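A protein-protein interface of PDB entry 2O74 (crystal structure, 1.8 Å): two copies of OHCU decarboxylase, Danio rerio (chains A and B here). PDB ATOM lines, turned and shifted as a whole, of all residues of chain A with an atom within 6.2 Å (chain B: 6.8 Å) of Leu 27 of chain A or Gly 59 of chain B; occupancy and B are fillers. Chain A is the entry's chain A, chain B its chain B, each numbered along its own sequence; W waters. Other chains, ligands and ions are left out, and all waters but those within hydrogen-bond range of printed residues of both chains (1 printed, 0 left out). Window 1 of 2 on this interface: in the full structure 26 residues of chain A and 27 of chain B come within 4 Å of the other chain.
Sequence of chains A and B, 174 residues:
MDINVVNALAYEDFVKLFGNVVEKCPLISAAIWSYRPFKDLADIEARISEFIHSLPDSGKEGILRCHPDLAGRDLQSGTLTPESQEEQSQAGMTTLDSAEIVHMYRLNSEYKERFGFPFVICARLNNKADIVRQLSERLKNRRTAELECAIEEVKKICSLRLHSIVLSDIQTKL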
ATOM      1  N   GLY A  19      22.768   9.858  38.508  1.00  0.00           N
ATOM      2  CA  GLY A  19      22.472  11.286  38.296  1.00  0.00           C
ATOM      3  C   GLY A  19      22.882  12.246  39.406  1.00  0.00           C
ATOM      4  O   GLY A  19      22.907  13.458  39.200  1.00  0.00           O
ATOM      5  N   LYS A  24      23.684  17.572  42.238  1.00  0.00           N
ATOM      6  CA  LYS A  24      22.699  18.309  41.429  1.00  0.00           C
ATOM      7  C   LYS A  24      23.169  18.528  39.984  1.00  0.00           C
ATOM      8  O   LYS A  24      22.774  19.496  39.321  1.00  0.00           O
ATOM      9  CB  LYS A  24      22.313  19.633  42.107  1.00  0.00           C
ATOM     10  CG  LYS A  24      21.822  19.428  43.549  1.00  0.00           C
ATOM     11  CD  LYS A  24      21.010  20.613  44.056  1.00  0.00           C
ATOM     12  CE  LYS A  24      20.770  20.484  45.554  1.00  0.00           C
ATOM     13  NZ  LYS A  24      19.706  21.402  46.032  1.00  0.00           N
ATOM     14  N   CYS A  25      24.006  17.616  39.505  1.00  0.00           N
ATOM     15  CA  CYS A  25      24.532  17.694  38.151  1.00  0.00           C
ATOM     16  C   CYS A  25      24.287  16.393  37.363  1.00  0.00           C
ATOM     17  O   CYS A  25      25.244  15.741  36.911  1.00  0.00           O
ATOM     18  CB  CYS A  25      26.026  18.017  38.187  1.00  0.00           C
ATOM     19  SG  CYS A  25      26.416  19.688  38.755  1.00  0.00           S
ATOM     20  N   PRO A  26      23.009  16.026  37.167  1.00  0.00           N
ATOM     21  CA  PRO A  26      22.694  14.804  36.404  1.00  0.00           C
ATOM     22  C   PRO A  26      23.222  14.857  34.977  1.00  0.00           C
ATOM     23  O   PRO A  26      23.441  13.817  34.342  1.00  0.00           O
ATOM     24  CB  PRO A  26      21.156  14.764  36.421  1.00  0.00           C
ATOM     25  CG  PRO A  26      20.740  16.175  36.633  1.00  0.00           C
ATOM     26  CD  PRO A  26      21.787  16.711  37.613  1.00  0.00           C
ATOM     27  N   LEU A  27      23.437  16.074  34.493  1.00  0.00           N
ATOM     28  CA  LEU A  27      23.972  16.302  33.181  1.00  0.00           C
ATOM     29  C   LEU A  27      25.278  15.544  32.959  1.00  0.00           C
ATOM     30  O   LEU A  27      25.545  15.010  31.874  1.00  0.00           O
ATOM     31  CB  LEU A  27      24.190  17.803  32.993  1.00  0.00           C
ATOM     32  CG  LEU A  27      25.013  18.149  31.761  1.00  0.00           C
ATOM     33  CD1 LEU A  27      24.300  17.559  30.545  1.00  0.00           C
ATOM     34  CD2 LEU A  27      25.129  19.639  31.661  1.00  0.00           C
ATOM     35  N   ILE A  28      26.094  15.486  33.996  1.00  0.00           N
ATOM     36  CA  ILE A  28      27.380  14.807  33.882  1.00  0.00           C
ATOM     37  C   ILE A  28      27.200  13.303  33.687  1.00  0.00           C
ATOM     38  O   ILE A  28      27.799  12.722  32.784  1.00  0.00           O
ATOM     39  CB  ILE A  28      28.285  15.126  35.076  1.00  0.00           C
ATOM     40  CG1 ILE A  28      28.631  16.619  35.061  1.00  0.00           C
ATOM     41  CG2 ILE A  28      29.550  14.241  35.053  1.00  0.00           C
ATOM     42  CD1 ILE A  28      29.163  17.121  36.406  1.00  0.00           C
ATOM     43  N   SER A  29      26.364  12.679  34.505  1.00  0.00           N
ATOM     44  CA  SER A  29      26.056  11.267  34.317  1.00  0.00           C
ATOM     45  C   SER A  29      25.372  11.029  32.949  1.00  0.00           C
ATOM     46  O   SER A  29      25.732  10.095  32.218  1.00  0.00           O
ATOM     47  CB  SER A  29      25.207  10.724  35.477  1.00  0.00           C
ATOM     48  OG  SER A  29      23.832  11.043  35.346  1.00  0.00           O
ATOM     49  N   ALA A  30      24.424  11.895  32.600  1.00  0.00           N
ATOM     50  CA  ALA A  30      23.732  11.815  31.312  1.00  0.00           C
ATOM     51  C   ALA A  30      24.718  11.858  30.139  1.00  0.00           C
ATOM     52  O   ALA A  30      24.612  11.044  29.207  1.00  0.00           O
ATOM     53  CB  ALA A  30      22.670  12.918  31.188  1.00  0.00           C
ATOM     54  N   ALA A  31      25.688  12.775  30.185  1.00  0.00           N
ATOM     55  CA  ALA A  31      26.663  12.895  29.110  1.00  0.00           C
ATOM     56  C   ALA A  31      27.523  11.653  28.981  1.00  0.00           C
ATOM     57  O   ALA A  31      27.669  11.102  27.885  1.00  0.00           O
ATOM     58  CB  ALA A  31      27.566  14.129  29.295  1.00  0.00           C
ATOM     59  N   ILE A  32      28.083  11.185  30.095  1.00  0.00           N
ATOM     60  CA  ILE A  32      29.060  10.107  29.996  1.00  0.00           C
ATOM     61  C   ILE A  32      28.471   8.805  29.451  1.00  0.00           C
ATOM     62  O   ILE A  32      29.211   7.983  28.935  1.00  0.00           O
ATOM     63  CB  ILE A  32      29.838   9.835  31.313  1.00  0.00           C
ATOM     64  CG1 ILE A  32      28.884   9.429  32.445  1.00  0.00           C
ATOM     65  CG2 ILE A  32      30.744  11.030  31.639  1.00  0.00           C
ATOM     66  CD1 ILE A  32      29.585   8.732  33.641  1.00  0.00           C
ATOM     67  N   TYR A  35      29.505   7.348  26.134  1.00  0.00           N
ATOM     68  CA  TYR A  35      30.795   6.703  25.957  1.00  0.00           C
ATOM     69  C   TYR A  35      30.774   5.199  26.321  1.00  0.00           C
ATOM     70  O   TYR A  35      31.806   4.544  26.350  1.00  0.00           O
ATOM     71  CB  TYR A  35      31.867   7.451  26.773  1.00  0.00           C
ATOM     72  CG  TYR A  35      32.038   8.915  26.379  1.00  0.00           C
ATOM     73  CD1 TYR A  35      32.724   9.277  25.222  1.00  0.00           C
ATOM     74  CD2 TYR A  35      31.487   9.931  27.153  1.00  0.00           C
ATOM     75  CE1 TYR A  35      32.870  10.619  24.858  1.00  0.00           C
ATOM     76  CE2 TYR A  35      31.637  11.275  26.798  1.00  0.00           C
ATOM     77  CZ  TYR A  35      32.318  11.609  25.657  1.00  0.00           C
ATOM     78  OH  TYR A  35      32.465  12.939  25.317  1.00  0.00           O
ATOM     79  N   PHE A  51      35.191  14.972  31.325  1.00  0.00           N
ATOM     80  CA  PHE A  51      34.064  15.844  31.013  1.00  0.00           C
ATOM     81  C   PHE A  51      34.194  17.164  31.765  1.00  0.00           C
ATOM     82  O   PHE A  51      34.052  18.245  31.194  1.00  0.00           O
ATOM     83  CB  PHE A  51      32.731  15.186  31.357  1.00  0.00           C
ATOM     84  CG  PHE A  51      31.547  15.991  30.908  1.00  0.00           C
ATOM     85  CD1 PHE A  51      31.117  15.931  29.582  1.00  0.00           C
ATOM     86  CD2 PHE A  51      30.877  16.828  31.793  1.00  0.00           C
ATOM     87  CE1 PHE A  51      30.037  16.697  29.162  1.00  0.00           C
ATOM     88  CE2 PHE A  51      29.789  17.598  31.378  1.00  0.00           C
ATOM     89  CZ  PHE A  51      29.371  17.524  30.069  1.00  0.00           C
ATOM     90  N   LYS B  24      16.638  20.690  34.357  1.00  0.00           N
ATOM     91  CA  LYS B  24      17.459  19.877  35.274  1.00  0.00           C
ATOM     92  C   LYS B  24      18.959  20.099  35.125  1.00  0.00           C
ATOM     93  O   LYS B  24      19.772  19.268  35.561  1.00  0.00           O
ATOM     94  CB  LYS B  24      17.077  18.391  35.185  1.00  0.00           C
ATOM     95  CG  LYS B  24      15.742  18.112  35.882  1.00  0.00           C
ATOM     96  CD  LYS B  24      15.297  16.653  35.846  1.00  0.00           C
ATOM     97  CE  LYS B  24      13.878  16.507  36.455  1.00  0.00           C
ATOM     98  NZ  LYS B  24      13.479  15.081  36.713  1.00  0.00           N
ATOM     99  N   CYS B  25      19.319  21.240  34.541  1.00  0.00           N
ATOM    100  CA  CYS B  25      20.725  21.622  34.393  1.00  0.00           C
ATOM    101  C   CYS B  25      21.102  22.955  35.072  1.00  0.00           C
ATOM    102  O   CYS B  25      21.544  23.903  34.399  1.00  0.00           O
ATOM    103  CB  CYS B  25      21.094  21.696  32.911  1.00  0.00           C
ATOM    104  SG  CYS B  25      20.955  20.111  32.022  1.00  0.00           S
ATOM    105  N   LEU B  27      23.623  23.711  36.646  1.00  0.00           N
ATOM    106  CA  LEU B  27      25.040  23.989  36.446  1.00  0.00           C
ATOM    107  C   LEU B  27      25.252  25.060  35.367  1.00  0.00           C
ATOM    108  O   LEU B  27      26.148  25.916  35.462  1.00  0.00           O
ATOM    109  CB  LEU B  27      25.742  22.708  36.010  1.00  0.00           C
ATOM    110  CG  LEU B  27      26.948  23.165  35.212  1.00  0.00           C
ATOM    111  CD1 LEU B  27      28.087  23.312  36.215  1.00  0.00           C
ATOM    112  CD2 LEU B  27      27.322  22.280  34.054  1.00  0.00           C
ATOM    113  N   ILE B  28      24.408  25.025  34.347  1.00  0.00           N
ATOM    114  CA  ILE B  28      24.543  25.955  33.223  1.00  0.00           C
ATOM    115  C   ILE B  28      24.230  27.403  33.635  1.00  0.00           C
ATOM    116  O   ILE B  28      25.017  28.320  33.383  1.00  0.00           O
ATOM    117  CB  ILE B  28      23.691  25.490  32.023  1.00  0.00           C
ATOM    118  CG1 ILE B  28      24.123  24.068  31.609  1.00  0.00           C
ATOM    119  CG2 ILE B  28      23.823  26.466  30.863  1.00  0.00           C
ATOM    120  CD1 ILE B  28      23.540  23.585  30.308  1.00  0.00           C
ATOM    121  N   PHE B  51      27.640  28.832  26.189  1.00  0.00           N
ATOM    122  CA  PHE B  51      28.060  27.773  27.099  1.00  0.00           C
ATOM    123  C   PHE B  51      27.674  26.391  26.528  1.00  0.00           C
ATOM    124  O   PHE B  51      28.517  25.481  26.423  1.00  0.00           O
ATOM    125  CB  PHE B  51      27.472  27.968  28.500  1.00  0.00           C
ATOM    126  CG  PHE B  51      27.983  26.972  29.493  1.00  0.00           C
ATOM    127  CD1 PHE B  51      29.066  27.280  30.310  1.00  0.00           C
ATOM    128  CD2 PHE B  51      27.394  25.719  29.607  1.00  0.00           C
ATOM    129  CE1 PHE B  51      29.554  26.338  31.211  1.00  0.00           C
ATOM    130  CE2 PHE B  51      27.886  24.761  30.512  1.00  0.00           C
ATOM    131  CZ  PHE B  51      28.957  25.078  31.316  1.00  0.00           C
ATOM    132  N   ILE B  52      26.416  26.253  26.118  1.00  0.00           N
ATOM    133  CA  ILE B  52      25.935  24.992  25.545  1.00  0.00           C
ATOM    134  C   ILE B  52      26.811  24.638  24.342  1.00  0.00           C
ATOM    135  O   ILE B  52      27.251  23.501  24.161  1.00  0.00           O
ATOM    136  CB  ILE B  52      24.445  25.102  25.109  1.00  0.00           C
ATOM    137  CG1 ILE B  52      23.519  25.276  26.330  1.00  0.00           C
ATOM    138  CG2 ILE B  52      24.048  23.895  24.238  1.00  0.00           C
ATOM    139  CD1 ILE B  52      22.028  25.588  26.004  1.00  0.00           C
ATOM    140  N   LEU B  55      30.166  22.915  24.858  1.00  0.00           N
ATOM    141  CA  LEU B  55      30.131  21.533  25.351  1.00  0.00           C
ATOM    142  C   LEU B  55      30.532  20.508  24.299  1.00  0.00           C
ATOM    143  O   LEU B  55      30.301  20.709  23.110  1.00  0.00           O
ATOM    144  CB  LEU B  55      28.723  21.184  25.842  1.00  0.00           C
ATOM    145  CG  LEU B  55      28.196  21.922  27.070  1.00  0.00           C
ATOM    146  CD1 LEU B  55      26.791  21.403  27.454  1.00  0.00           C
ATOM    147  CD2 LEU B  55      29.135  21.801  28.267  1.00  0.00           C
ATOM    148  N   PRO B  56      31.106  19.379  24.740  1.00  0.00           N
ATOM    149  CA  PRO B  56      31.292  18.286  23.796  1.00  0.00           C
ATOM    150  C   PRO B  56      29.922  17.808  23.348  1.00  0.00           C
ATOM    151  O   PRO B  56      28.926  18.107  24.007  1.00  0.00           O
ATOM    152  CB  PRO B  56      31.992  17.197  24.623  1.00  0.00           C
ATOM    153  CG  PRO B  56      31.961  17.616  26.010  1.00  0.00           C
ATOM    154  CD  PRO B  56      31.615  19.072  26.086  1.00  0.00           C
ATOM    155  N   ASP B  57      29.869  17.080  22.239  1.00  0.00           N
ATOM    156  CA  ASP B  57      28.619  16.469  21.793  1.00  0.00           C
ATOM    157  C   ASP B  57      27.930  15.665  22.907  1.00  0.00           C
ATOM    158  O   ASP B  57      26.705  15.715  23.047  1.00  0.00           O
ATOM    159  CB  ASP B  57      28.855  15.590  20.565  1.00  0.00           C
ATOM    160  CG  ASP B  57      28.956  16.400  19.277  1.00  0.00           C
ATOM    161  OD1 ASP B  57      28.881  17.652  19.344  1.00  0.00           O
ATOM    162  OD2 ASP B  57      29.097  15.772  18.196  1.00  0.00           O
ATOM    163  N   SER B  58      28.712  14.910  23.681  1.00  0.00           N
ATOM    164  CA  SER B  58      28.155  14.148  24.798  1.00  0.00           C
ATOM    165  C   SER B  58      27.444  15.077  25.780  1.00  0.00           C
ATOM    166  O   SER B  58      26.447  14.708  26.377  1.00  0.00           O
ATOM    167  CB  SER B  58      29.248  13.364  25.548  1.00  0.00           C
ATOM    168  OG  SER B  58      30.243  14.237  26.091  1.00  0.00           O
ATOM    169  N   GLY B  59      27.971  16.284  25.938  1.00  0.00           N
ATOM    170  CA  GLY B  59      27.372  17.270  26.836  1.00  0.00           C
ATOM    171  C   GLY B  59      26.018  17.714  26.309  1.00  0.00           C
ATOM    172  O   GLY B  59      25.078  17.912  27.085  1.00  0.00           O
ATOM    173  N   LYS B  60      25.930  17.884  24.990  1.00  0.00           N
ATOM    174  CA  LYS B  60      24.673  18.270  24.346  1.00  0.00           C
ATOM    175  C   LYS B  60      23.646  17.128  24.460  1.00  0.00           C
ATOM    176  O   LYS B  60      22.507  17.345  24.857  1.00  0.00           O
ATOM    177  CB  LYS B  60      24.931  18.671  22.892  1.00  0.00           C
ATOM    178  CG  LYS B  60      25.780  19.953  22.783  1.00  0.00           C
ATOM    179  CD  LYS B  60      26.252  20.215  21.359  1.00  0.00           C
ATOM    180  CE  LYS B  60      26.885  21.594  21.251  1.00  0.00           C
ATOM    181  NZ  LYS B  60      27.144  21.919  19.815  1.00  0.00           N
ATOM    182  N   GLU B  61      24.065  15.920  24.112  1.00  0.00           N
ATOM    183  CA  GLU B  61      23.242  14.728  24.333  1.00  0.00           C
ATOM    184  C   GLU B  61      22.813  14.627  25.792  1.00  0.00           C
ATOM    185  O   GLU B  61      21.674  14.258  26.093  1.00  0.00           O
ATOM    186  CB  GLU B  61      24.027  13.479  23.944  1.00  0.00           C
ATOM    187  CG  GLU B  61      24.408  13.432  22.479  1.00  0.00           C
ATOM    188  CD  GLU B  61      25.288  12.234  22.125  1.00  0.00           C
ATOM    189  OE1 GLU B  61      26.304  12.000  22.819  1.00  0.00           O
ATOM    190  OE2 GLU B  61      24.969  11.539  21.130  1.00  0.00           O
ATOM    191  N   GLY B  62      23.725  14.941  26.711  1.00  0.00           N
ATOM    192  CA  GLY B  62      23.392  14.900  28.135  1.00  0.00           C
ATOM    193  C   GLY B  62      22.283  15.859  28.529  1.00  0.00           C
ATOM    194  O   GLY B  62      21.381  15.500  29.307  1.00  0.00           O
ATOM    195  N   ILE B  63      22.349  17.085  28.012  1.00  0.00           N
ATOM    196  CA  ILE B  63      21.279  18.062  28.243  1.00  0.00           C
ATOM    197  C   ILE B  63      19.948  17.486  27.774  1.00  0.00           C
ATOM    198  O   ILE B  63      18.971  17.553  28.490  1.00  0.00           O
ATOM    199  CB  ILE B  63      21.555  19.393  27.523  1.00  0.00           C
ATOM    200  CG1 ILE B  63      22.772  20.062  28.165  1.00  0.00           C
ATOM    201  CG2 ILE B  63      20.305  20.306  27.537  1.00  0.00           C
ATOM    202  CD1 ILE B  63      23.298  21.248  27.403  1.00  0.00           C
ATOM    203  N   LEU B  64      19.941  16.879  26.595  1.00  0.00           N
ATOM    204  CA  LEU B  64      18.719  16.296  26.048  1.00  0.00           C
ATOM    205  C   LEU B  64      18.151  15.218  26.984  1.00  0.00           C
ATOM    206  O   LEU B  64      16.940  15.208  27.300  1.00  0.00           O
ATOM    207  CB  LEU B  64      18.972  15.749  24.643  1.00  0.00           C
ATOM    208  CG  LEU B  64      19.271  16.809  23.575  1.00  0.00           C
ATOM    209  CD1 LEU B  64      19.782  16.153  22.302  1.00  0.00           C
ATOM    210  CD2 LEU B  64      18.031  17.643  23.333  1.00  0.00           C
ATOM    211  N   ARG B  65      19.038  14.355  27.461  1.00  0.00           N
ATOM    212  CA  ARG B  65      18.671  13.246  28.344  1.00  0.00           C
ATOM    213  C   ARG B  65      18.093  13.698  29.688  1.00  0.00           C
ATOM    214  O   ARG B  65      17.459  12.906  30.403  1.00  0.00           O
ATOM    215  CB  ARG B  65      19.864  12.281  28.537  1.00  0.00           C
ATOM    216  CG  ARG B  65      20.237  11.482  27.279  1.00  0.00           C
ATOM    217  CD  ARG B  65      21.586  10.786  27.425  1.00  0.00           C
ATOM    218  NE  ARG B  65      22.030  10.254  26.143  1.00  0.00           N
ATOM    219  CZ  ARG B  65      23.288  10.229  25.725  1.00  0.00           C
ATOM    220  NH1 ARG B  65      24.265  10.722  26.495  1.00  0.00           N
ATOM    221  NH2 ARG B  65      23.563   9.723  24.517  1.00  0.00           N
ATOM    222  N   CYS B  66      18.325  14.963  30.033  1.00  0.00           N
ATOM    223  CA  CYS B  66      17.762  15.559  31.221  1.00  0.00           C
ATOM    224  C   CYS B  66      16.323  16.050  31.024  1.00  0.00           C
ATOM    225  O   CYS B  66      15.704  16.523  31.977  1.00  0.00           O
ATOM    226  CB  CYS B  66      18.645  16.731  31.704  1.00  0.00           C
ATOM    227  SG  CYS B  66      20.207  16.205  32.412  1.00  0.00           S
ATOM    228  N   ILE B 151      19.181  20.497  19.872  1.00  0.00           N
ATOM    229  CA  ILE B 151      19.761  21.539  20.738  1.00  0.00           C
ATOM    230  C   ILE B 151      19.149  22.909  20.459  1.00  0.00           C
ATOM    231  O   ILE B 151      18.977  23.718  21.371  1.00  0.00           O
ATOM    232  CB  ILE B 151      21.300  21.600  20.579  1.00  0.00           C
ATOM    233  CG1 ILE B 151      21.950  20.355  21.209  1.00  0.00           C
ATOM    234  CG2 ILE B 151      21.896  22.918  21.186  1.00  0.00           C
ATOM    235  CD1 ILE B 151      21.665  20.167  22.712  1.00  0.00           C
HETATM  236  O   HOH W   1      31.501  13.962  22.897  1.00  0.00           O
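Of the 19 printed residues of chain B, 8 touch a printed residue of chain A.
Hydrophobic or aromatic side chains of chain A that line the printed part of chain B: Pro 26, Leu 27, Ala 30, Ala 31, Tyr 35 and Phe 51.
CG of Pro 26 of chain A touches O of Lys 24 of chain B, at 3.4 Å.
Leu 27 of chain A touches Gly 59 of chain B.
Gly 62 of chain B touches Leu 27 of chain A.
CD1 of Leu 27 of chain A touches N of Ile 63 of chain B, at 3.2 Å.
Ala 30 of chain A touches Gly 62 of chain B.
Ser 58 of chain B touches Ala 31 of chain A (O to CB, 3.2 Å).
Ala 31 of chain A touches Gly 59 of chain B.
Ala 31 of chain A touches Gly 62 of chain B (N to CA, 3.7 Å).
CE1 of Phe 51 of chain A touches CG of Pro 56 of chain B, at 3.8 Å.
CE1 of Phe 51 of chain A touches CA of Gly 59 of chain B, 3.6 Å away.
NH1 of Arg 65 of chain B lies within hydrogen-bond range of O of Ala 30 of chain A (2.8 Å).
OH of Tyr 35 of chain A lies within hydrogen-bond range of OG of Ser 58 of chain B (2.7 Å).
O of Pro 26 of chain A is in hydrogen-bond range of OG of Ser 29 of chain A (3.0 Å).
The side-chain carboxylate (OE1) of Glu 61 of chain B is in salt-bridge range of the guanidinium group (NH2) of Arg 65 of chain B (3.9 Å).
The backbone carbonyl oxygen of Gly 62 of chain B sits at hydrogen-bond distance from the side-chain sulfur of Cys 66 of chain B, at 3.4 Å.
Water W1 lies within hydrogen-bond range of the side-chain hydroxyl (OH) of Tyr 35 of chain A (2.8 Å) and the backbone NH (N) of Ser 58 of chain B (3.0 Å).
Positions printed for both chains: 24, 25, 27, 28 and 51.
Of the 15 pairs that touch across the chains among the printed residues, none has its exchanged pair printed and touching as well.
Of the printed residues of chain A, Gly 59 of chain B touches Leu 27 (3.6 Å), Ala 31 (3.99 Å) and Phe 51 (3.6 Å).
Printed residues of chain A within 4 Å of Pro 56 of chain B: Phe 51 (3.8 Å).
Of the printed residues of chain A, Arg 65 of chain B touches Ala 30 (2.8 Å) and Ala 31 (3.7 Å).
Printed residues of chain A within 4 Å of Ile 63 of chain B: Leu 27.
Ile 28 of chain A touches none of the printed residues of chain B.
The nearest printed residue of chain A that does not touch Gly 59 of chain B is Tyr 35 of chain A (5.6 Å).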
